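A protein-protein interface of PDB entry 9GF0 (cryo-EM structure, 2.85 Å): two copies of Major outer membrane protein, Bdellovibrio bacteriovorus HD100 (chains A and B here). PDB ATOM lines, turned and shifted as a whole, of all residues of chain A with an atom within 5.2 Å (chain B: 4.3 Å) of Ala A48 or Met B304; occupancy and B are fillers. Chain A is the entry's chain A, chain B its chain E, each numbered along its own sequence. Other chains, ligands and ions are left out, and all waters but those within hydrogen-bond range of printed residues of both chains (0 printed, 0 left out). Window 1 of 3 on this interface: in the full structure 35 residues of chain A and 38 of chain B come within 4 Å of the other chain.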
ATOM      1  N   ILE A  36     -11.870   4.964 -15.306  1.00  0.00           N
ATOM      2  CA  ILE A  36     -12.495   6.057 -14.569  1.00  0.00           C
ATOM      3  C   ILE A  36     -13.959   5.705 -14.342  1.00  0.00           C
ATOM      4  O   ILE A  36     -14.679   5.377 -15.290  1.00  0.00           O
ATOM      5  CB  ILE A  36     -12.360   7.404 -15.306  1.00  0.00           C
ATOM      6  CG1 ILE A  36     -10.891   7.808 -15.419  1.00  0.00           C
ATOM      7  CG2 ILE A  36     -13.089   8.488 -14.554  1.00  0.00           C
ATOM      8  CD1 ILE A  36     -10.431   8.072 -16.821  1.00  0.00           C
ATOM      9  N   GLU A  37     -14.391   5.773 -13.085  1.00  0.00           N
ATOM     10  CA  GLU A  37     -15.761   5.469 -12.692  1.00  0.00           C
ATOM     11  C   GLU A  37     -16.519   6.774 -12.494  1.00  0.00           C
ATOM     12  O   GLU A  37     -16.137   7.593 -11.654  1.00  0.00           O
ATOM     13  CB  GLU A  37     -15.781   4.637 -11.411  1.00  0.00           C
ATOM     14  CG  GLU A  37     -17.065   3.869 -11.182  1.00  0.00           C
ATOM     15  CD  GLU A  37     -17.000   2.467 -11.734  1.00  0.00           C
ATOM     16  OE1 GLU A  37     -15.908   1.867 -11.687  1.00  0.00           O
ATOM     17  OE2 GLU A  37     -18.034   1.967 -12.221  1.00  0.00           O
ATOM     18  N   TRP A  38     -17.598   6.952 -13.251  1.00  0.00           N
ATOM     19  CA  TRP A  38     -18.305   8.224 -13.276  1.00  0.00           C
ATOM     20  C   TRP A  38     -19.112   8.435 -12.004  1.00  0.00           C
ATOM     21  O   TRP A  38     -19.736   7.509 -11.486  1.00  0.00           O
ATOM     22  CB  TRP A  38     -19.235   8.288 -14.483  1.00  0.00           C
ATOM     23  CG  TRP A  38     -18.559   8.195 -15.815  1.00  0.00           C
ATOM     24  CD1 TRP A  38     -17.327   7.680 -16.085  1.00  0.00           C
ATOM     25  CD2 TRP A  38     -19.099   8.614 -17.068  1.00  0.00           C
ATOM     26  NE1 TRP A  38     -17.060   7.771 -17.424  1.00  0.00           N
ATOM     27  CE2 TRP A  38     -18.137   8.334 -18.051  1.00  0.00           C
ATOM     28  CE3 TRP A  38     -20.305   9.199 -17.455  1.00  0.00           C
ATOM     29  CZ2 TRP A  38     -18.342   8.622 -19.390  1.00  0.00           C
ATOM     30  CZ3 TRP A  38     -20.499   9.487 -18.776  1.00  0.00           C
ATOM     31  CH2 TRP A  38     -19.530   9.194 -19.732  1.00  0.00           C
ATOM     32  N   GLY A  39     -19.115   9.667 -11.509  1.00  0.00           N
ATOM     33  CA  GLY A  39     -19.887   9.983 -10.327  1.00  0.00           C
ATOM     34  C   GLY A  39     -19.592  11.388  -9.848  1.00  0.00           C
ATOM     35  O   GLY A  39     -18.918  12.167 -10.523  1.00  0.00           O
ATOM     36  N   ASN A  40     -20.111  11.692  -8.665  1.00  0.00           N
ATOM     37  CA  ASN A  40     -19.952  12.993  -8.040  1.00  0.00           C
ATOM     38  C   ASN A  40     -18.938  12.918  -6.899  1.00  0.00           C
ATOM     39  O   ASN A  40     -18.276  11.901  -6.684  1.00  0.00           O
ATOM     40  CB  ASN A  40     -21.303  13.506  -7.553  1.00  0.00           C
ATOM     41  CG  ASN A  40     -21.364  15.012  -7.503  1.00  0.00           C
ATOM     42  OD1 ASN A  40     -20.337  15.681  -7.473  1.00  0.00           O
ATOM     43  ND2 ASN A  40     -22.570  15.554  -7.484  1.00  0.00           N
ATOM     44  N   PRO A  46     -23.704   7.368  -7.636  1.00  0.00           N
ATOM     45  CA  PRO A  46     -22.325   6.866  -7.665  1.00  0.00           C
ATOM     46  C   PRO A  46     -21.270   7.902  -7.304  1.00  0.00           C
ATOM     47  O   PRO A  46     -21.476   9.104  -7.408  1.00  0.00           O
ATOM     48  CB  PRO A  46     -22.172   6.392  -9.112  1.00  0.00           C
ATOM     49  CG  PRO A  46     -23.086   7.260  -9.881  1.00  0.00           C
ATOM     50  CD  PRO A  46     -24.271   7.464  -8.988  1.00  0.00           C
ATOM     51  N   HIS A  47     -20.119   7.414  -6.860  1.00  0.00           N
ATOM     52  CA  HIS A  47     -18.973   8.224  -6.487  1.00  0.00           C
ATOM     53  C   HIS A  47     -17.944   8.195  -7.610  1.00  0.00           C
ATOM     54  O   HIS A  47     -17.872   7.235  -8.380  1.00  0.00           O
ATOM     55  CB  HIS A  47     -18.360   7.700  -5.187  1.00  0.00           C
ATOM     56  CG  HIS A  47     -17.456   8.672  -4.495  1.00  0.00           C
ATOM     57  ND1 HIS A  47     -16.213   8.318  -4.021  1.00  0.00           N
ATOM     58  CD2 HIS A  47     -17.618   9.978  -4.189  1.00  0.00           C
ATOM     59  CE1 HIS A  47     -15.646   9.366  -3.454  1.00  0.00           C
ATOM     60  NE2 HIS A  47     -16.476  10.387  -3.544  1.00  0.00           N
ATOM     61  N   ALA A  48     -17.155   9.260  -7.709  1.00  0.00           N
ATOM     62  CA  ALA A  48     -16.145   9.371  -8.752  1.00  0.00           C
ATOM     63  C   ALA A  48     -14.877   8.644  -8.321  1.00  0.00           C
ATOM     64  O   ALA A  48     -14.332   8.923  -7.251  1.00  0.00           O
ATOM     65  CB  ALA A  48     -15.852  10.836  -9.048  1.00  0.00           C
ATOM     66  N   GLU A  49     -14.418   7.699  -9.143  1.00  0.00           N
ATOM     67  CA  GLU A  49     -13.228   6.914  -8.847  1.00  0.00           C
ATOM     68  C   GLU A  49     -12.472   6.607 -10.131  1.00  0.00           C
ATOM     69  O   GLU A  49     -13.055   6.561 -11.214  1.00  0.00           O
ATOM     70  CB  GLU A  49     -13.566   5.599  -8.135  1.00  0.00           C
ATOM     71  CG  GLU A  49     -14.657   5.690  -7.081  1.00  0.00           C
ATOM     72  CD  GLU A  49     -15.086   4.341  -6.567  1.00  0.00           C
ATOM     73  OE1 GLU A  49     -14.700   3.328  -7.181  1.00  0.00           O
ATOM     74  OE2 GLU A  49     -15.801   4.291  -5.545  1.00  0.00           O
ATOM     75  N   GLY A  50     -11.166   6.388  -9.997  1.00  0.00           N
ATOM     76  CA  GLY A  50     -10.332   6.079 -11.145  1.00  0.00           C
ATOM     77  C   GLY A  50      -8.906   5.701 -10.794  1.00  0.00           C
ATOM     78  O   GLY A  50      -8.393   6.105  -9.750  1.00  0.00           O
ATOM     79  N   PHE A  66      -8.010   6.063  -6.981  1.00  0.00           N
ATOM     80  CA  PHE A  66      -8.553   7.181  -6.221  1.00  0.00           C
ATOM     81  C   PHE A  66     -10.032   6.953  -5.962  1.00  0.00           C
ATOM     82  O   PHE A  66     -10.787   6.667  -6.893  1.00  0.00           O
ATOM     83  CB  PHE A  66      -8.373   8.505  -6.966  1.00  0.00           C
ATOM     84  CG  PHE A  66      -6.950   8.928  -7.124  1.00  0.00           C
ATOM     85  CD1 PHE A  66      -5.965   8.422  -6.298  1.00  0.00           C
ATOM     86  CD2 PHE A  66      -6.597   9.834  -8.100  1.00  0.00           C
ATOM     87  CE1 PHE A  66      -4.657   8.806  -6.450  1.00  0.00           C
ATOM     88  CE2 PHE A  66      -5.293  10.224  -8.253  1.00  0.00           C
ATOM     89  CZ  PHE A  66      -4.320   9.708  -7.425  1.00  0.00           C
ATOM     90  N   GLY A  67     -10.440   7.091  -4.706  1.00  0.00           N
ATOM     91  CA  GLY A  67     -11.842   7.194  -4.369  1.00  0.00           C
ATOM     92  C   GLY A  67     -12.565   5.908  -4.050  1.00  0.00           C
ATOM     93  O   GLY A  67     -13.793   5.934  -3.923  1.00  0.00           O
ATOM     94  N   SER B 278     -11.044  12.182 -17.234  1.00  0.00           N
ATOM     95  CA  SER B 278      -9.999  12.401 -16.245  1.00  0.00           C
ATOM     96  C   SER B 278     -10.590  12.258 -14.850  1.00  0.00           C
ATOM     97  O   SER B 278     -11.803  12.353 -14.656  1.00  0.00           O
ATOM     98  CB  SER B 278      -9.344  13.775 -16.416  1.00  0.00           C
ATOM     99  OG  SER B 278     -10.272  14.815 -16.178  1.00  0.00           O
ATOM    100  N   THR B 302     -12.469  13.714  -4.566  1.00  0.00           N
ATOM    101  CA  THR B 302     -12.356  12.991  -5.825  1.00  0.00           C
ATOM    102  C   THR B 302     -13.424  13.471  -6.799  1.00  0.00           C
ATOM    103  O   THR B 302     -14.603  13.574  -6.449  1.00  0.00           O
ATOM    104  CB  THR B 302     -12.478  11.487  -5.602  1.00  0.00           C
ATOM    105  OG1 THR B 302     -11.870  11.141  -4.356  1.00  0.00           O
ATOM    106  CG2 THR B 302     -11.770  10.747  -6.706  1.00  0.00           C
ATOM    107  N   ARG B 303     -13.006  13.770  -8.025  1.00  0.00           N
ATOM    108  CA  ARG B 303     -13.881  14.355  -9.025  1.00  0.00           C
ATOM    109  C   ARG B 303     -13.478  13.836 -10.393  1.00  0.00           C
ATOM    110  O   ARG B 303     -12.340  13.415 -10.610  1.00  0.00           O
ATOM    111  CB  ARG B 303     -13.810  15.883  -8.996  1.00  0.00           C
ATOM    112  CG  ARG B 303     -12.390  16.390  -8.880  1.00  0.00           C
ATOM    113  CD  ARG B 303     -12.267  17.867  -9.178  1.00  0.00           C
ATOM    114  NE  ARG B 303     -10.871  18.284  -9.257  1.00  0.00           N
ATOM    115  CZ  ARG B 303     -10.028  18.302  -8.233  1.00  0.00           C
ATOM    116  NH1 ARG B 303     -10.409  17.952  -7.016  1.00  0.00           N
ATOM    117  NH2 ARG B 303      -8.771  18.683  -8.434  1.00  0.00           N
ATOM    118  N   MET B 304     -14.423  13.879 -11.324  1.00  0.00           N
ATOM    119  CA  MET B 304     -14.168  13.428 -12.679  1.00  0.00           C
ATOM    120  C   MET B 304     -14.845  14.355 -13.676  1.00  0.00           C
ATOM    121  O   MET B 304     -15.776  15.093 -13.344  1.00  0.00           O
ATOM    122  CB  MET B 304     -14.648  11.990 -12.901  1.00  0.00           C
ATOM    123  CG  MET B 304     -16.138  11.781 -12.724  1.00  0.00           C
ATOM    124  SD  MET B 304     -16.968  11.776 -14.312  1.00  0.00           S
ATOM    125  CE  MET B 304     -16.054  10.482 -15.114  1.00  0.00           C
ATOM    126  N   ALA B 305     -14.357  14.307 -14.913  1.00  0.00           N
ATOM    127  CA  ALA B 305     -14.956  15.023 -16.026  1.00  0.00           C
ATOM    128  C   ALA B 305     -14.898  14.144 -17.263  1.00  0.00           C
ATOM    129  O   ALA B 305     -13.889  13.481 -17.514  1.00  0.00           O
ATOM    130  CB  ALA B 305     -14.246  16.352 -16.290  1.00  0.00           C
ATOM    131  N   SER B 324     -22.550  12.862 -16.417  1.00  0.00           N
ATOM    132  CA  SER B 324     -21.386  12.222 -15.812  1.00  0.00           C
ATOM    133  C   SER B 324     -21.434  12.310 -14.294  1.00  0.00           C
ATOM    134  O   SER B 324     -21.001  11.388 -13.598  1.00  0.00           O
ATOM    135  CB  SER B 324     -20.102  12.851 -16.340  1.00  0.00           C
ATOM    136  OG  SER B 324     -19.654  13.874 -15.476  1.00  0.00           O
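No position is printed for both chains.
Met B304 touches just these residues of chain A: Ile A36, Trp A38, Gly A39 and Ala A48. Printed residues of chain B within 4 Å of Gly A67: Thr B302. Printed residues of chain B within 4 Å of Trp A38: Met B304 (3.2 Å) and Ser B324 (3.6 Å). Of the printed residues of chain A, Thr B302 touches Ala A48 and Gly A67. Printed residues of chain B within 4 Å of Gly A39: Met B304 and Ser B324. Arg B303 touches none of the printed residues of chain A. The nearest residue of chain B that does not touch Ala A48 is Arg B303 (4.03 Å). The nearest printed residue of chain B that does not touch Ile A36 is Ser B278 (4.1 Å).
SD of Met B304 lies within hydrogen-bond range of OG of Ser B324, 3.6 Å away. The backbone carbonyl oxygen of Asn A40 is in hydrogen-bond range of the backbone NH of Ala A48, 3.0 Å away. ND1 of His A47 is in hydrogen-bond range of O of Gly A67 (3.4 Å).
Of the 6 printed residues of chain B, 3 touch a printed residue of chain A. Printed residues of chain B that touch a printed residue of chain A: Thr B302, Met B304 and Ser B324. Of the 12 printed residues of chain A, 5 touch a printed residue of chain B. Hydrophobic or aromatic side chains of chain A within 4 Å of the printed part of chain B: Ile A36, Trp A38 and Ala A48. Among the printed residues, no Asp or Glu carboxylate lies within 4 Å of a Lys or Arg side-chain nitrogen of the other chain.
The backbone NH (N) of Gly A39 is in hydrogen-bond range of the backbone carbonyl oxygen (O) of Ser B324 (3.3 Å).
Among the printed residues, merely in contact across the chains: Ile A36 with Met B304 (3.6 Å), Trp A38 with Met B304 (3.2 Å), Trp A38 with Ser B324 (3.6 Å), Gly A39 with Met B304 (3.6 Å), Ala A48 with Thr B302 (3.2 Å), Ala A48 with Met B304 (3.8 Å) and Gly A67 with Thr B302 (3.9 Å).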
